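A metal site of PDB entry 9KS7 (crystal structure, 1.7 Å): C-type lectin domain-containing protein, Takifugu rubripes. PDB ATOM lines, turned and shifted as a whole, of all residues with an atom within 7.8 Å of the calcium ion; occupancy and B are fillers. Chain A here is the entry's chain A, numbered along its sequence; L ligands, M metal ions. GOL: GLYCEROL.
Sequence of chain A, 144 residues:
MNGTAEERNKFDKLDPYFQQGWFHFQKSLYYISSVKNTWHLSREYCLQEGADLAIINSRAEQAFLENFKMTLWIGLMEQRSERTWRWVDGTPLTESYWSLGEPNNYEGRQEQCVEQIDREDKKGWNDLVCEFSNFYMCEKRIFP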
ATOM      1  N   ARG A  83      14.830  13.188 -19.568  1.00  0.00           N
ATOM      2  CA  ARG A  83      14.394  14.554 -19.325  1.00  0.00           C
ATOM      3  C   ARG A  83      14.444  14.862 -17.835  1.00  0.00           C
ATOM      4  O   ARG A  83      13.632  15.629 -17.306  1.00  0.00           O
ATOM      5  CB  ARG A  83      12.991  14.801 -19.899  1.00  0.00           C
ATOM      6  CG  ARG A  83      12.898  14.589 -21.435  1.00  0.00           C
ATOM      7  CD  ARG A  83      13.200  15.883 -22.206  1.00  0.00           C
ATOM      8  NE  ARG A  83      14.649  16.113 -22.371  1.00  0.00           N
ATOM      9  CZ  ARG A  83      15.154  17.180 -22.973  1.00  0.00           C
ATOM     10  NH1 ARG A  83      14.385  18.196 -23.332  1.00  0.00           N
ATOM     11  NH2 ARG A  83      16.458  17.232 -23.251  1.00  0.00           N
ATOM     12  N   TRP A  98      15.670  27.672 -16.395  1.00  0.00           N
ATOM     13  CA  TRP A  98      15.422  27.439 -17.810  1.00  0.00           C
ATOM     14  C   TRP A  98      14.844  28.677 -18.488  1.00  0.00           C
ATOM     15  O   TRP A  98      13.999  29.379 -17.920  1.00  0.00           O
ATOM     16  CB  TRP A  98      14.421  26.290 -17.991  1.00  0.00           C
ATOM     17  CG  TRP A  98      14.880  24.946 -17.505  1.00  0.00           C
ATOM     18  CD1 TRP A  98      14.403  24.259 -16.405  1.00  0.00           C
ATOM     19  CD2 TRP A  98      15.876  24.112 -18.113  1.00  0.00           C
ATOM     20  NE1 TRP A  98      15.068  23.047 -16.290  1.00  0.00           N
ATOM     21  CE2 TRP A  98      15.960  22.934 -17.332  1.00  0.00           C
ATOM     22  CE3 TRP A  98      16.693  24.243 -19.244  1.00  0.00           C
ATOM     23  CZ2 TRP A  98      16.854  21.897 -17.634  1.00  0.00           C
ATOM     24  CZ3 TRP A  98      17.575  23.195 -19.555  1.00  0.00           C
ATOM     25  CH2 TRP A  98      17.654  22.032 -18.748  1.00  0.00           C
ATOM     26  N   SER A  99      15.287  28.948 -19.714  1.00  0.00           N
ATOM     27  CA  SER A  99      14.645  30.024 -20.461  1.00  0.00           C
ATOM     28  C   SER A  99      13.254  29.563 -20.900  1.00  0.00           C
ATOM     29  O   SER A  99      12.936  28.375 -20.923  1.00  0.00           O
ATOM     30  CB  SER A  99      15.468  30.440 -21.670  1.00  0.00           C
ATOM     31  OG  SER A  99      15.855  29.334 -22.474  1.00  0.00           O
ATOM     32  N   GLY A 101      10.121  28.196 -22.428  1.00  0.00           N
ATOM     33  CA  GLY A 101       9.907  27.121 -23.383  1.00  0.00           C
ATOM     34  C   GLY A 101      10.944  26.010 -23.351  1.00  0.00           C
ATOM     35  O   GLY A 101      10.838  25.067 -24.150  1.00  0.00           O
ATOM     36  N   GLU A 102      11.937  26.085 -22.468  1.00  0.00           N
ATOM     37  CA  GLU A 102      12.992  25.088 -22.375  1.00  0.00           C
ATOM     38  C   GLU A 102      12.859  24.276 -21.079  1.00  0.00           C
ATOM     39  O   GLU A 102      12.251  24.731 -20.107  1.00  0.00           O
ATOM     40  CB  GLU A 102      14.381  25.759 -22.414  1.00  0.00           C
ATOM     41  CG  GLU A 102      14.614  26.691 -23.607  1.00  0.00           C
ATOM     42  CD  GLU A 102      14.646  25.986 -24.952  1.00  0.00           C
ATOM     43  OE1 GLU A 102      14.837  24.738 -24.963  1.00  0.00           O
ATOM     44  OE2 GLU A 102      14.512  26.672 -26.004  1.00  0.00           O
ATOM     45  N   PRO A 103      13.418  23.050 -21.040  1.00  0.00           N
ATOM     46  CA  PRO A 103      14.127  22.358 -22.130  1.00  0.00           C
ATOM     47  C   PRO A 103      13.132  21.762 -23.100  1.00  0.00           C
ATOM     48  O   PRO A 103      12.002  21.454 -22.689  1.00  0.00           O
ATOM     49  CB  PRO A 103      14.925  21.279 -21.385  1.00  0.00           C
ATOM     50  CG  PRO A 103      14.021  20.925 -20.200  1.00  0.00           C
ATOM     51  CD  PRO A 103      13.358  22.243 -19.808  1.00  0.00           C
ATOM     52  N   ASN A 104      13.497  21.565 -24.373  1.00  0.00           N
ATOM     53  CA  ASN A 104      12.499  21.201 -25.367  1.00  0.00           C
ATOM     54  C   ASN A 104      12.883  20.154 -26.415  1.00  0.00           C
ATOM     55  O   ASN A 104      12.023  19.831 -27.234  1.00  0.00           O
ATOM     56  CB  ASN A 104      12.024  22.477 -26.096  1.00  0.00           C
ATOM     57  CG  ASN A 104      13.115  23.097 -26.956  1.00  0.00           C
ATOM     58  OD1 ASN A 104      14.262  22.627 -26.935  1.00  0.00           O
ATOM     59  ND2 ASN A 104      12.763  24.105 -27.740  1.00  0.00           N
ATOM     60  N   ASN A 105      14.105  19.601 -26.426  1.00  0.00           N
ATOM     61  CA  ASN A 105      14.487  18.675 -27.513  1.00  0.00           C
ATOM     62  C   ASN A 105      14.042  19.234 -28.863  1.00  0.00           C
ATOM     63  O   ASN A 105      13.278  18.616 -29.629  1.00  0.00           O
ATOM     64  CB  ASN A 105      13.908  17.262 -27.307  1.00  0.00           C
ATOM     65  CG  ASN A 105      14.745  16.406 -26.353  1.00  0.00           C
ATOM     66  OD1 ASN A 105      15.961  16.547 -26.274  1.00  0.00           O
ATOM     67  ND2 ASN A 105      14.076  15.529 -25.600  1.00  0.00           N
ATOM     68  N   TYR A 106      14.542  20.433 -29.149  1.00  0.00           N
ATOM     69  CA  TYR A 106      14.056  21.262 -30.238  1.00  0.00           C
ATOM     70  C   TYR A 106      13.989  20.481 -31.549  1.00  0.00           C
ATOM     71  O   TYR A 106      14.947  19.803 -31.934  1.00  0.00           O
ATOM     72  CB  TYR A 106      14.989  22.466 -30.383  1.00  0.00           C
ATOM     73  CG  TYR A 106      14.603  23.481 -31.438  1.00  0.00           C
ATOM     74  CD1 TYR A 106      13.410  24.175 -31.377  1.00  0.00           C
ATOM     75  CD2 TYR A 106      15.471  23.741 -32.498  1.00  0.00           C
ATOM     76  CE1 TYR A 106      13.080  25.110 -32.345  1.00  0.00           C
ATOM     77  CE2 TYR A 106      15.152  24.669 -33.472  1.00  0.00           C
ATOM     78  CZ  TYR A 106      13.959  25.348 -33.391  1.00  0.00           C
ATOM     79  OH  TYR A 106      13.650  26.269 -34.370  1.00  0.00           O
ATOM     80  N   GLU A 107      12.839  20.575 -32.221  1.00  0.00           N
ATOM     81  CA  GLU A 107      12.620  19.921 -33.527  1.00  0.00           C
ATOM     82  C   GLU A 107      12.857  18.419 -33.470  1.00  0.00           C
ATOM     83  O   GLU A 107      13.179  17.791 -34.492  1.00  0.00           O
ATOM     84  CB  GLU A 107      13.488  20.570 -34.616  1.00  0.00           C
ATOM     85  CG  GLU A 107      13.139  22.038 -34.804  1.00  0.00           C
ATOM     86  CD  GLU A 107      13.854  22.649 -35.995  1.00  0.00           C
ATOM     87  OE1 GLU A 107      15.026  22.296 -36.223  1.00  0.00           O
ATOM     88  OE2 GLU A 107      13.253  23.509 -36.667  1.00  0.00           O
ATOM     89  N   ARG A 109      15.236  16.767 -31.973  1.00  0.00           N
ATOM     90  CA  ARG A 109      16.593  16.260 -31.894  1.00  0.00           C
ATOM     91  C   ARG A 109      16.999  16.127 -30.430  1.00  0.00           C
ATOM     92  O   ARG A 109      16.396  16.733 -29.540  1.00  0.00           O
ATOM     93  CB  ARG A 109      17.547  17.159 -32.670  1.00  0.00           C
ATOM     94  CG  ARG A 109      17.733  18.491 -32.033  1.00  0.00           C
ATOM     95  CD  ARG A 109      18.119  19.547 -33.046  1.00  0.00           C
ATOM     96  NE  ARG A 109      18.205  20.816 -32.340  1.00  0.00           N
ATOM     97  CZ  ARG A 109      18.841  21.893 -32.779  1.00  0.00           C
ATOM     98  NH1 ARG A 109      19.231  21.999 -34.046  1.00  0.00           N
ATOM     99  NH2 ARG A 109      19.063  22.889 -31.936  1.00  0.00           N
ATOM    100  N   GLU A 111      18.735  16.849 -27.307  1.00  0.00           N
ATOM    101  CA  GLU A 111      19.430  17.996 -26.707  1.00  0.00           C
ATOM    102  C   GLU A 111      19.711  17.646 -25.248  1.00  0.00           C
ATOM    103  O   GLU A 111      18.898  17.947 -24.359  1.00  0.00           O
ATOM    104  CB  GLU A 111      18.586  19.265 -26.847  1.00  0.00           C
ATOM    105  CG  GLU A 111      18.421  19.686 -28.304  1.00  0.00           C
ATOM    106  CD  GLU A 111      17.841  21.094 -28.443  1.00  0.00           C
ATOM    107  OE1 GLU A 111      16.854  21.416 -27.750  1.00  0.00           O
ATOM    108  OE2 GLU A 111      18.387  21.871 -29.264  1.00  0.00           O
ATOM    109  N   CYS A 113      22.611  18.474 -23.401  1.00  0.00           N
ATOM    110  CA  CYS A 113      23.562  19.306 -22.667  1.00  0.00           C
ATOM    111  C   CYS A 113      23.005  20.714 -22.476  1.00  0.00           C
ATOM    112  O   CYS A 113      22.184  21.175 -23.256  1.00  0.00           O
ATOM    113  CB  CYS A 113      24.892  19.357 -23.429  1.00  0.00           C
ATOM    114  SG  CYS A 113      25.766  17.757 -23.367  1.00  0.00           S
ATOM    115  N   GLU A 115      23.274  24.842 -21.993  1.00  0.00           N
ATOM    116  CA  GLU A 115      23.968  26.117 -22.135  1.00  0.00           C
ATOM    117  C   GLU A 115      23.161  27.215 -21.444  1.00  0.00           C
ATOM    118  O   GLU A 115      21.937  27.134 -21.315  1.00  0.00           O
ATOM    119  CB  GLU A 115      24.141  26.505 -23.600  1.00  0.00           C
ATOM    120  CG  GLU A 115      22.794  26.670 -24.331  1.00  0.00           C
ATOM    121  CD  GLU A 115      22.889  27.133 -25.775  1.00  0.00           C
ATOM    122  OE1 GLU A 115      24.014  27.346 -26.285  1.00  0.00           O
ATOM    123  OE2 GLU A 115      21.809  27.314 -26.412  1.00  0.00           O
ATOM    124  N   ILE A 117      21.924  30.620 -22.449  1.00  0.00           N
ATOM    125  CA  ILE A 117      21.822  31.276 -23.739  1.00  0.00           C
ATOM    126  C   ILE A 117      21.647  32.767 -23.484  1.00  0.00           C
ATOM    127  O   ILE A 117      21.017  33.186 -22.507  1.00  0.00           O
ATOM    128  CB  ILE A 117      20.692  30.664 -24.586  1.00  0.00           C
ATOM    129  CG1 ILE A 117      20.750  31.211 -26.014  1.00  0.00           C
ATOM    130  CG2 ILE A 117      19.323  30.949 -23.984  1.00  0.00           C
ATOM    131  CD1 ILE A 117      19.779  30.502 -26.965  1.00  0.00           C
ATOM    132  N   LYS A 122      15.494  36.451 -24.929  1.00  0.00           N
ATOM    133  CA  LYS A 122      15.473  35.141 -24.295  1.00  0.00           C
ATOM    134  C   LYS A 122      16.777  34.922 -23.541  1.00  0.00           C
ATOM    135  O   LYS A 122      17.844  34.921 -24.163  1.00  0.00           O
ATOM    136  CB  LYS A 122      15.270  34.060 -25.365  1.00  0.00           C
ATOM    137  CG  LYS A 122      14.840  32.706 -24.865  1.00  0.00           C
ATOM    138  CD  LYS A 122      15.084  31.626 -25.922  1.00  0.00           C
ATOM    139  CE  LYS A 122      14.562  30.260 -25.494  1.00  0.00           C
ATOM    140  NZ  LYS A 122      15.556  29.188 -25.845  1.00  0.00           N
ATOM    141  N   TRP A 125      18.696  29.070 -19.157  1.00  0.00           N
ATOM    142  CA  TRP A 125      19.270  27.814 -19.622  1.00  0.00           C
ATOM    143  C   TRP A 125      18.521  27.280 -20.846  1.00  0.00           C
ATOM    144  O   TRP A 125      17.301  27.460 -20.981  1.00  0.00           O
ATOM    145  CB  TRP A 125      19.228  26.730 -18.544  1.00  0.00           C
ATOM    146  CG  TRP A 125      19.882  27.079 -17.258  1.00  0.00           C
ATOM    147  CD1 TRP A 125      20.726  28.112 -16.991  1.00  0.00           C
ATOM    148  CD2 TRP A 125      19.730  26.342 -16.043  1.00  0.00           C
ATOM    149  NE1 TRP A 125      21.110  28.074 -15.658  1.00  0.00           N
ATOM    150  CE2 TRP A 125      20.518  26.983 -15.065  1.00  0.00           C
ATOM    151  CE3 TRP A 125      19.015  25.176 -15.692  1.00  0.00           C
ATOM    152  CZ2 TRP A 125      20.595  26.504 -13.753  1.00  0.00           C
ATOM    153  CZ3 TRP A 125      19.083  24.727 -14.383  1.00  0.00           C
ATOM    154  CH2 TRP A 125      19.869  25.374 -13.436  1.00  0.00           C
ATOM    155  N   ASN A 126      19.258  26.578 -21.708  1.00  0.00           N
ATOM    156  CA  ASN A 126      18.665  25.910 -22.852  1.00  0.00           C
ATOM    157  C   ASN A 126      19.307  24.540 -22.999  1.00  0.00           C
ATOM    158  O   ASN A 126      20.528  24.410 -22.857  1.00  0.00           O
ATOM    159  CB  ASN A 126      18.867  26.759 -24.118  1.00  0.00           C
ATOM    160  CG  ASN A 126      18.466  26.024 -25.377  1.00  0.00           C
ATOM    161  OD1 ASN A 126      17.358  25.489 -25.465  1.00  0.00           O
ATOM    162  ND2 ASN A 126      19.370  25.987 -26.370  1.00  0.00           N
ATOM    163  N   ASP A 127      18.500  23.502 -23.261  1.00  0.00           N
ATOM    164  CA  ASP A 127      19.089  22.242 -23.689  1.00  0.00           C
ATOM    165  C   ASP A 127      19.483  22.317 -25.160  1.00  0.00           C
ATOM    166  O   ASP A 127      18.748  22.867 -25.999  1.00  0.00           O
ATOM    167  CB  ASP A 127      18.136  21.056 -23.445  1.00  0.00           C
ATOM    168  CG  ASP A 127      16.812  21.146 -24.195  1.00  0.00           C
ATOM    169  OD1 ASP A 127      16.341  22.264 -24.495  1.00  0.00           O
ATOM    170  OD2 ASP A 127      16.209  20.064 -24.420  1.00  0.00           O
ATOM    171  N   LEU A 128      20.648  21.763 -25.476  1.00  0.00           N
ATOM    172  CA  LEU A 128      21.203  21.873 -26.826  1.00  0.00           C
ATOM    173  C   LEU A 128      21.943  20.590 -27.170  1.00  0.00           C
ATOM    174  O   LEU A 128      22.395  19.859 -26.295  1.00  0.00           O
ATOM    175  CB  LEU A 128      22.157  23.088 -26.913  1.00  0.00           C
ATOM    176  CG  LEU A 128      22.682  23.437 -28.297  1.00  0.00           C
ATOM    177  CD1 LEU A 128      21.531  23.977 -29.131  1.00  0.00           C
ATOM    178  CD2 LEU A 128      23.823  24.495 -28.211  1.00  0.00           C
ATOM    179  N   VAL A 129      22.060  20.315 -28.476  1.00  0.00           N
ATOM    180  CA  VAL A 129      22.855  19.176 -28.924  1.00  0.00           C
ATOM    181  C   VAL A 129      24.281  19.270 -28.382  1.00  0.00           C
ATOM    182  O   VAL A 129      24.947  20.294 -28.532  1.00  0.00           O
ATOM    183  CB  VAL A 129      22.865  19.126 -30.462  1.00  0.00           C
ATOM    184  CG1 VAL A 129      23.714  17.941 -30.940  1.00  0.00           C
ATOM    185  CG2 VAL A 129      21.419  19.037 -30.994  1.00  0.00           C
HETATM  186  C1  GOL L   1      17.348  25.125 -29.408  1.00  0.00           C
HETATM  187  O1  GOL L   1      17.890  24.319 -28.385  1.00  0.00           O
HETATM  188  C2  GOL L   1      16.087  25.856 -28.972  1.00  0.00           C
HETATM  189  O2  GOL L   1      15.375  25.286 -27.887  1.00  0.00           O
HETATM  190  C3  GOL L   1      16.127  27.372 -29.072  1.00  0.00           C
HETATM  191  O3  GOL L   1      14.800  27.804 -29.316  1.00  0.00           O
HETATM  192 CA    CA M   1      16.459  23.564 -26.481  1.00  0.00          CA
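OD1 of Asn 126 is bound to the calcium ion (2.4 Å).
The calcium ion is bound by the side-chain carboxylate (OD1) of Asp 127 (2.4 Å).
OD1 of Asn 104 binds the calcium ion, at 2.4 Å.
O of Asp 127 binds the calcium ion, at 2.4 Å.
O2 of the ligand binds the calcium ion.
O1 of the ligand binds the calcium ion (2.5 Å).
OE1 of Glu 102 is bound to the calcium ion (2.5 Å).
The calcium ion is bound by OE1 of Glu 111 (2.5 Å).
Five residues have an atom within 4 Å of the calcium ion: Glu 102, Asn 104, Glu 111, Asn 126 and Asp 127.
The nearest printed residue that does not touch the calcium ion is Tyr 106 (4.3 Å).
OD2 of Asp 127 is in hydrogen-bond range of N of Asn 105 (2.9 Å).
The guanidinium group of Arg 83 lies within salt-bridge range of the side-chain carboxylate of Asp 127 (2.8 Å).
The side-chain amide oxygen of Asn 104 sits close to the backbone NH of Tyr 106 (3.1 Å).
NZ of Lys 122 is in salt-bridge range of OE2 of Glu 102.
N of Tyr 106 sits close to OE1 of Glu 111, 2.9 Å away.
The side-chain amide oxygen (OD1) of Asn 105 is in hydrogen-bond range of the backbone NH (N) of Glu 111 (3.0 Å).
The side-chain carboxylate (OE2) of Glu 111 lies within salt-bridge range of the guanidinium group (NH2) of Arg 109 (2.9 Å).
The backbone carbonyl oxygen (O) of Glu 111 lies within hydrogen-bond range of the guanidinium group (NH2) of Arg 83, 2.8 Å away.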
